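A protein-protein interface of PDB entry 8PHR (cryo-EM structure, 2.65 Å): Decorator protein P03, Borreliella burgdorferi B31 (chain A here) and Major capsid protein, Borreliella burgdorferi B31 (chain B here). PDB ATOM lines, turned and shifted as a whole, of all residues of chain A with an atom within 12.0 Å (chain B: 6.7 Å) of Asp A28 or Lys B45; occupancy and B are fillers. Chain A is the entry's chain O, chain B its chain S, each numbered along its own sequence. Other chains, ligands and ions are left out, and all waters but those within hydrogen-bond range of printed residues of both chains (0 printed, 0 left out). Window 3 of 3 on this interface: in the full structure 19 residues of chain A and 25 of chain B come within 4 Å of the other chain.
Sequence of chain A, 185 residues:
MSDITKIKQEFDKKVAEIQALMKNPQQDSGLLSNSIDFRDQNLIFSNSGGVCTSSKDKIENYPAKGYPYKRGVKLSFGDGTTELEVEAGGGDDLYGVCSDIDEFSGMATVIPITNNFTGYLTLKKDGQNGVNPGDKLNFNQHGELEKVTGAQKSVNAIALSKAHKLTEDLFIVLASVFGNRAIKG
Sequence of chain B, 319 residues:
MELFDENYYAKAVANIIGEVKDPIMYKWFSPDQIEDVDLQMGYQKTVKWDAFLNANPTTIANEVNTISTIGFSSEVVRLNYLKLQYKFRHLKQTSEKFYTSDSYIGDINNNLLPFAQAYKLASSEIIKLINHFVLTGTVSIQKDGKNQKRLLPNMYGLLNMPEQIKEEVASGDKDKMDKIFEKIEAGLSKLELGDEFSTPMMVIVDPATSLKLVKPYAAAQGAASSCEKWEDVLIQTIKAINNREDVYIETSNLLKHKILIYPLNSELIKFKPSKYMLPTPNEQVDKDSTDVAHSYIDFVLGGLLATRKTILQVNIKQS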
ATOM      1  N   MET A  22     -29.600 -26.059 -24.936  1.00  0.00           N
ATOM      2  CA  MET A  22     -28.170 -26.155 -24.677  1.00  0.00           C
ATOM      3  C   MET A  22     -27.878 -27.485 -24.000  1.00  0.00           C
ATOM      4  O   MET A  22     -28.620 -27.903 -23.105  1.00  0.00           O
ATOM      5  CB  MET A  22     -27.685 -24.995 -23.799  1.00  0.00           C
ATOM      6  CG  MET A  22     -27.525 -23.671 -24.532  1.00  0.00           C
ATOM      7  SD  MET A  22     -26.067 -23.631 -25.594  1.00  0.00           S
ATOM      8  CE  MET A  22     -26.818 -23.470 -27.211  1.00  0.00           C
ATOM      9  N   LYS A  23     -26.808 -28.152 -24.439  1.00  0.00           N
ATOM     10  CA  LYS A  23     -26.423 -29.422 -23.831  1.00  0.00           C
ATOM     11  C   LYS A  23     -26.144 -29.251 -22.342  1.00  0.00           C
ATOM     12  O   LYS A  23     -26.656 -30.008 -21.510  1.00  0.00           O
ATOM     13  CB  LYS A  23     -25.201 -29.997 -24.551  1.00  0.00           C
ATOM     14  CG  LYS A  23     -24.447 -31.056 -23.762  1.00  0.00           C
ATOM     15  CD  LYS A  23     -23.134 -31.414 -24.437  1.00  0.00           C
ATOM     16  CE  LYS A  23     -22.298 -32.341 -23.568  1.00  0.00           C
ATOM     17  NZ  LYS A  23     -20.975 -32.635 -24.186  1.00  0.00           N
ATOM     18  N   ASN A  24     -25.330 -28.257 -21.991  1.00  0.00           N
ATOM     19  CA  ASN A  24     -25.108 -27.897 -20.599  1.00  0.00           C
ATOM     20  C   ASN A  24     -26.001 -26.717 -20.256  1.00  0.00           C
ATOM     21  O   ASN A  24     -25.923 -25.685 -20.941  1.00  0.00           O
ATOM     22  CB  ASN A  24     -23.644 -27.544 -20.363  1.00  0.00           C
ATOM     23  CG  ASN A  24     -23.296 -27.435 -18.890  1.00  0.00           C
ATOM     24  OD1 ASN A  24     -24.145 -27.626 -18.020  1.00  0.00           O
ATOM     25  ND2 ASN A  24     -22.037 -27.126 -18.604  1.00  0.00           N
ATOM     26  N   PRO A  25     -26.870 -26.823 -19.251  1.00  0.00           N
ATOM     27  CA  PRO A  25     -27.757 -25.700 -18.918  1.00  0.00           C
ATOM     28  C   PRO A  25     -26.972 -24.424 -18.647  1.00  0.00           C
ATOM     29  O   PRO A  25     -25.963 -24.430 -17.937  1.00  0.00           O
ATOM     30  CB  PRO A  25     -28.488 -26.192 -17.665  1.00  0.00           C
ATOM     31  CG  PRO A  25     -28.511 -27.675 -17.815  1.00  0.00           C
ATOM     32  CD  PRO A  25     -27.226 -28.049 -18.512  1.00  0.00           C
ATOM     33  N   GLN A  26     -27.450 -23.320 -19.226  1.00  0.00           N
ATOM     34  CA  GLN A  26     -26.742 -22.049 -19.111  1.00  0.00           C
ATOM     35  C   GLN A  26     -26.801 -21.511 -17.687  1.00  0.00           C
ATOM     36  O   GLN A  26     -25.795 -21.033 -17.151  1.00  0.00           O
ATOM     37  CB  GLN A  26     -27.325 -21.036 -20.097  1.00  0.00           C
ATOM     38  CG  GLN A  26     -27.516 -21.581 -21.504  1.00  0.00           C
ATOM     39  CD  GLN A  26     -28.098 -20.553 -22.453  1.00  0.00           C
ATOM     40  OE1 GLN A  26     -27.489 -20.213 -23.468  1.00  0.00           O
ATOM     41  NE2 GLN A  26     -29.284 -20.053 -22.129  1.00  0.00           N
ATOM     42  N   GLN A  27     -27.974 -21.572 -17.061  1.00  0.00           N
ATOM     43  CA  GLN A  27     -28.125 -21.066 -15.705  1.00  0.00           C
ATOM     44  C   GLN A  27     -27.355 -21.942 -14.725  1.00  0.00           C
ATOM     45  O   GLN A  27     -27.498 -23.168 -14.725  1.00  0.00           O
ATOM     46  CB  GLN A  27     -29.602 -21.011 -15.320  1.00  0.00           C
ATOM     47  CG  GLN A  27     -30.459 -20.185 -16.265  1.00  0.00           C
ATOM     48  CD  GLN A  27     -31.934 -20.245 -15.918  1.00  0.00           C
ATOM     49  OE1 GLN A  27     -32.332 -20.907 -14.960  1.00  0.00           O
ATOM     50  NE2 GLN A  27     -32.754 -19.553 -16.701  1.00  0.00           N
ATOM     51  N   ASP A  28     -26.532 -21.309 -13.894  1.00  0.00           N
ATOM     52  CA  ASP A  28     -25.781 -22.041 -12.886  1.00  0.00           C
ATOM     53  C   ASP A  28     -26.722 -22.581 -11.815  1.00  0.00           C
ATOM     54  O   ASP A  28     -27.661 -21.902 -11.391  1.00  0.00           O
ATOM     55  CB  ASP A  28     -24.721 -21.142 -12.253  1.00  0.00           C
ATOM     56  CG  ASP A  28     -23.677 -20.678 -13.250  1.00  0.00           C
ATOM     57  OD1 ASP A  28     -23.805 -21.016 -14.446  1.00  0.00           O
ATOM     58  OD2 ASP A  28     -22.729 -19.977 -12.839  1.00  0.00           O
ATOM     59  N   SER A  29     -26.467 -23.812 -11.384  1.00  0.00           N
ATOM     60  CA  SER A  29     -27.296 -24.428 -10.359  1.00  0.00           C
ATOM     61  C   SER A  29     -27.106 -23.718  -9.026  1.00  0.00           C
ATOM     62  O   SER A  29     -26.010 -23.258  -8.696  1.00  0.00           O
ATOM     63  CB  SER A  29     -26.954 -25.910 -10.216  1.00  0.00           C
ATOM     64  OG  SER A  29     -25.646 -26.076  -9.701  1.00  0.00           O
ATOM     65  N   GLY A  30     -28.192 -23.623  -8.255  1.00  0.00           N
ATOM     66  CA  GLY A  30     -28.123 -22.955  -6.969  1.00  0.00           C
ATOM     67  C   GLY A  30     -27.609 -23.811  -5.834  1.00  0.00           C
ATOM     68  O   GLY A  30     -27.183 -23.268  -4.810  1.00  0.00           O
ATOM     69  N   LEU A  31     -27.625 -25.135  -5.992  1.00  0.00           N
ATOM     70  CA  LEU A  31     -27.312 -26.051  -4.907  1.00  0.00           C
ATOM     71  C   LEU A  31     -26.322 -27.112  -5.366  1.00  0.00           C
ATOM     72  O   LEU A  31     -26.182 -27.393  -6.559  1.00  0.00           O
ATOM     73  CB  LEU A  31     -28.574 -26.735  -4.371  1.00  0.00           C
ATOM     74  CG  LEU A  31     -29.591 -25.840  -3.669  1.00  0.00           C
ATOM     75  CD1 LEU A  31     -30.612 -26.690  -2.946  1.00  0.00           C
ATOM     76  CD2 LEU A  31     -28.896 -24.899  -2.706  1.00  0.00           C
ATOM     77  N   LEU A  32     -25.632 -27.697  -4.389  1.00  0.00           N
ATOM     78  CA  LEU A  32     -24.757 -28.828  -4.650  1.00  0.00           C
ATOM     79  C   LEU A  32     -25.580 -30.085  -4.918  1.00  0.00           C
ATOM     80  O   LEU A  32     -26.733 -30.201  -4.497  1.00  0.00           O
ATOM     81  CB  LEU A  32     -23.821 -29.064  -3.465  1.00  0.00           C
ATOM     82  CG  LEU A  32     -22.777 -27.985  -3.169  1.00  0.00           C
ATOM     83  CD1 LEU A  32     -21.775 -28.478  -2.137  1.00  0.00           C
ATOM     84  CD2 LEU A  32     -22.071 -27.560  -4.442  1.00  0.00           C
ATOM     85  N   SER A  33     -24.973 -31.031  -5.626  1.00  0.00           N
ATOM     86  CA  SER A  33     -25.634 -32.284  -5.956  1.00  0.00           C
ATOM     87  C   SER A  33     -25.366 -33.336  -4.887  1.00  0.00           C
ATOM     88  O   SER A  33     -24.298 -33.369  -4.270  1.00  0.00           O
ATOM     89  CB  SER A  33     -25.169 -32.801  -7.317  1.00  0.00           C
ATOM     90  OG  SER A  33     -23.787 -33.114  -7.298  1.00  0.00           O
ATOM     91  N   GLU A 103     -19.755 -26.844 -28.350  1.00  0.00           N
ATOM     92  CA  GLU A 103     -20.411 -25.549 -28.501  1.00  0.00           C
ATOM     93  C   GLU A 103     -19.457 -24.491 -29.040  1.00  0.00           C
ATOM     94  O   GLU A 103     -19.856 -23.648 -29.853  1.00  0.00           O
ATOM     95  CB  GLU A 103     -20.997 -25.103 -27.161  1.00  0.00           C
ATOM     96  CG  GLU A 103     -22.008 -26.072 -26.571  1.00  0.00           C
ATOM     97  CD  GLU A 103     -22.294 -25.802 -25.106  1.00  0.00           C
ATOM     98  OE1 GLU A 103     -21.718 -24.842 -24.551  1.00  0.00           O
ATOM     99  OE2 GLU A 103     -23.094 -26.550 -24.507  1.00  0.00           O
ATOM    100  N   TYR B  43     -20.563 -12.373  -7.442  1.00  0.00           N
ATOM    101  CA  TYR B  43     -20.889 -13.786  -7.344  1.00  0.00           C
ATOM    102  C   TYR B  43     -19.615 -14.597  -7.153  1.00  0.00           C
ATOM    103  O   TYR B  43     -18.509 -14.145  -7.462  1.00  0.00           O
ATOM    104  CB  TYR B  43     -21.674 -14.262  -8.578  1.00  0.00           C
ATOM    105  CG  TYR B  43     -20.972 -14.073  -9.911  1.00  0.00           C
ATOM    106  CD1 TYR B  43     -19.873 -14.846 -10.267  1.00  0.00           C
ATOM    107  CD2 TYR B  43     -21.415 -13.113 -10.814  1.00  0.00           C
ATOM    108  CE1 TYR B  43     -19.237 -14.669 -11.481  1.00  0.00           C
ATOM    109  CE2 TYR B  43     -20.784 -12.930 -12.031  1.00  0.00           C
ATOM    110  CZ  TYR B  43     -19.696 -13.711 -12.359  1.00  0.00           C
ATOM    111  OH  TYR B  43     -19.065 -13.534 -13.568  1.00  0.00           O
ATOM    112  N   GLN B  44     -19.795 -15.806  -6.634  1.00  0.00           N
ATOM    113  CA  GLN B  44     -18.719 -16.774  -6.486  1.00  0.00           C
ATOM    114  C   GLN B  44     -19.177 -18.104  -7.063  1.00  0.00           C
ATOM    115  O   GLN B  44     -20.361 -18.441  -7.017  1.00  0.00           O
ATOM    116  CB  GLN B  44     -18.305 -16.942  -5.019  1.00  0.00           C
ATOM    117  CG  GLN B  44     -17.433 -15.814  -4.496  1.00  0.00           C
ATOM    118  CD  GLN B  44     -16.669 -16.197  -3.245  1.00  0.00           C
ATOM    119  OE1 GLN B  44     -16.841 -17.293  -2.710  1.00  0.00           O
ATOM    120  NE2 GLN B  44     -15.817 -15.295  -2.774  1.00  0.00           N
ATOM    121  N   LYS B  45     -18.231 -18.862  -7.612  1.00  0.00           N
ATOM    122  CA  LYS B  45     -18.557 -20.079  -8.339  1.00  0.00           C
ATOM    123  C   LYS B  45     -17.735 -21.250  -7.822  1.00  0.00           C
ATOM    124  O   LYS B  45     -16.600 -21.087  -7.367  1.00  0.00           O
ATOM    125  CB  LYS B  45     -18.321 -19.910  -9.846  1.00  0.00           C
ATOM    126  CG  LYS B  45     -19.324 -18.998 -10.533  1.00  0.00           C
ATOM    127  CD  LYS B  45     -19.087 -18.947 -12.033  1.00  0.00           C
ATOM    128  CE  LYS B  45     -20.058 -17.996 -12.714  1.00  0.00           C
ATOM    129  NZ  LYS B  45     -19.853 -17.956 -14.188  1.00  0.00           N
ATOM    130  N   THR B  46     -18.331 -22.438  -7.903  1.00  0.00           N
ATOM    131  CA  THR B  46     -17.657 -23.680  -7.553  1.00  0.00           C
ATOM    132  C   THR B  46     -18.106 -24.770  -8.517  1.00  0.00           C
ATOM    133  O   THR B  46     -19.175 -24.687  -9.126  1.00  0.00           O
ATOM    134  CB  THR B  46     -17.935 -24.097  -6.101  1.00  0.00           C
ATOM    135  OG1 THR B  46     -17.220 -25.302  -5.802  1.00  0.00           O
ATOM    136  CG2 THR B  46     -19.422 -24.326  -5.883  1.00  0.00           C
ATOM    137  N   VAL B  47     -17.269 -25.796  -8.657  1.00  0.00           N
ATOM    138  CA  VAL B  47     -17.473 -26.852  -9.642  1.00  0.00           C
ATOM    139  C   VAL B  47     -17.484 -28.198  -8.931  1.00  0.00           C
ATOM    140  O   VAL B  47     -16.591 -28.489  -8.128  1.00  0.00           O
ATOM    141  CB  VAL B  47     -16.386 -26.831 -10.734  1.00  0.00           C
ATOM    142  CG1 VAL B  47     -16.665 -27.897 -11.782  1.00  0.00           C
ATOM    143  CG2 VAL B  47     -16.299 -25.453 -11.373  1.00  0.00           C
ATOM    144  N   VAL B  76     -21.987 -26.483 -12.040  1.00  0.00           N
ATOM    145  CA  VAL B  76     -21.444 -25.200 -11.614  1.00  0.00           C
ATOM    146  C   VAL B  76     -22.457 -24.560 -10.677  1.00  0.00           C
ATOM    147  O   VAL B  76     -23.617 -24.351 -11.052  1.00  0.00           O
ATOM    148  CB  VAL B  76     -21.139 -24.286 -12.809  1.00  0.00           C
ATOM    149  CG1 VAL B  76     -20.605 -22.945 -12.328  1.00  0.00           C
ATOM    150  CG2 VAL B  76     -20.148 -24.955 -13.749  1.00  0.00           C
ATOM    151  N   VAL B  77     -22.021 -24.250  -9.459  1.00  0.00           N
ATOM    152  CA  VAL B  77     -22.875 -23.662  -8.435  1.00  0.00           C
ATOM    153  C   VAL B  77     -22.401 -22.240  -8.174  1.00  0.00           C
ATOM    154  O   VAL B  77     -21.215 -22.013  -7.903  1.00  0.00           O
ATOM    155  CB  VAL B  77     -22.865 -24.495  -7.144  1.00  0.00           C
ATOM    156  CG1 VAL B  77     -23.794 -23.879  -6.111  1.00  0.00           C
ATOM    157  CG2 VAL B  77     -23.268 -25.930  -7.441  1.00  0.00           C
ATOM    158  N   ARG B  78     -23.328 -21.289  -8.253  1.00  0.00           N
ATOM    159  CA  ARG B  78     -23.031 -19.874  -8.102  1.00  0.00           C
ATOM    160  C   ARG B  78     -23.788 -19.304  -6.910  1.00  0.00           C
ATOM    161  O   ARG B  78     -24.976 -19.583  -6.724  1.00  0.00           O
ATOM    162  CB  ARG B  78     -23.398 -19.095  -9.371  1.00  0.00           C
ATOM    163  CG  ARG B  78     -23.000 -17.629  -9.336  1.00  0.00           C
ATOM    164  CD  ARG B  78     -23.110 -16.991 -10.711  1.00  0.00           C
ATOM    165  NE  ARG B  78     -24.481 -16.991 -11.205  1.00  0.00           N
ATOM    166  CZ  ARG B  78     -25.135 -15.906 -11.598  1.00  0.00           C
ATOM    167  NH1 ARG B  78     -24.570 -14.709 -11.569  1.00  0.00           N
ATOM    168  NH2 ARG B  78     -26.387 -16.024 -12.030  1.00  0.00           N
ATOM    169  N   LEU B  79     -23.086 -18.513  -6.105  1.00  0.00           N
ATOM    170  CA  LEU B  79     -23.665 -17.793  -4.978  1.00  0.00           C
ATOM    171  C   LEU B  79     -23.578 -16.301  -5.266  1.00  0.00           C
ATOM    172  O   LEU B  79     -22.486 -15.779  -5.520  1.00  0.00           O
ATOM    173  CB  LEU B  79     -22.940 -18.135  -3.677  1.00  0.00           C
ATOM    174  CG  LEU B  79     -23.223 -19.509  -3.069  1.00  0.00           C
ATOM    175  CD1 LEU B  79     -22.597 -19.624  -1.688  1.00  0.00           C
ATOM    176  CD2 LEU B  79     -24.720 -19.773  -3.007  1.00  0.00           C
ATOM    177  N   ASN B 154     -30.185 -17.453  -7.140  1.00  0.00           N
ATOM    178  CA  ASN B 154     -29.165 -18.116  -6.324  1.00  0.00           C
ATOM    179  C   ASN B 154     -29.002 -17.434  -4.968  1.00  0.00           C
ATOM    180  O   ASN B 154     -27.917 -17.437  -4.383  1.00  0.00           O
ATOM    181  CB  ASN B 154     -27.820 -18.188  -7.054  1.00  0.00           C
ATOM    182  CG  ASN B 154     -27.852 -19.128  -8.242  1.00  0.00           C
ATOM    183  OD1 ASN B 154     -28.684 -18.986  -9.138  1.00  0.00           O
ATOM    184  ND2 ASN B 154     -26.941 -20.094  -8.257  1.00  0.00           N
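The backbone carbonyl oxygen (O) of Arg B78 is in hydrogen-bond range of the side-chain amide nitrogen (ND2) of Asn B154 (2.5 Å). The backbone NH (N) of Val B77 is in hydrogen-bond range of the backbone carbonyl oxygen (O) of Thr B46 (2.9 Å). The side-chain hydroxyl (OG) of Ser A29 sits at hydrogen-bond distance from the backbone carbonyl oxygen (O) of Leu A31, at 3.4 Å.
The backbone NH (N) of Arg B78 is in hydrogen-bond range of the backbone carbonyl oxygen (O) of Ser A29, at 3.4 Å. The backbone carbonyl oxygen (O) of Val B76 sits at hydrogen-bond distance from the backbone NH (N) of Ser A29, 2.9 Å away. The side-chain amino group (NZ) of Lys B45 lies within salt-bridge range of the side-chain carboxylate (OD2) of Asp A28, at 3.8 Å. The side-chain amide nitrogen of Asn B154 sits at hydrogen-bond distance from the backbone carbonyl oxygen of Ser A29 (3.3 Å). OD2 of Asp A28 is in salt-bridge range of NE of Arg B78 (3.8 Å).
Pro A25 touches none of the printed residues of chain B. Of chain B, only Lys B45, Val B76, Arg B78 and Asn B154 come within 4 Å of Asp A28. Of the printed residues of chain B, Gly A30 touches Val B77 and Asn B154. Of the printed residues of chain B, Leu A32 touches Val B77. No residue of chain A comes within 4 Å of Tyr B43. Of chain A, only Asp A28 (3.3 Å) comes within 4 Å of Lys B45. No residue of chain A comes within 4 Å of Val B47. Of chain A, only Asp A28 (3.6 Å) and Ser A29 (3.4 Å) come within 4 Å of Arg B78. The nearest residue of chain A that does not touch Lys B45 is Gln A26 (7.3 Å). The nearest printed residue of chain B that does not touch Ser A29 is Leu B79 (6.1 Å).
Among the printed residues, pairs that only touch across the chains: Asp A28 with Val B76 (3.6 Å), Asp A28 with Asn B154 (3.7 Å), Ser A29 with Val B77 (3.2 Å), Gly A30 with Val B77 (3.7 Å), Gly A30 with Asn B154 (3.4 Å), Leu A31 with Val B77 (3.4 Å) and Leu A32 with Val B77 (3.6 Å).
Along chain B the printed residues that touch a printed residue of chain A span positions 45 to 154. Hydrophobic or aromatic side chains of chain A within 4 Å of the printed part of chain B: Leu A32. Among the printed residues, Asp or Glu carboxylates within 4 Å of a Lys or Arg side-chain nitrogen of the other chain: Asp A28 with Lys B45 and Asp A28 with Arg B78.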
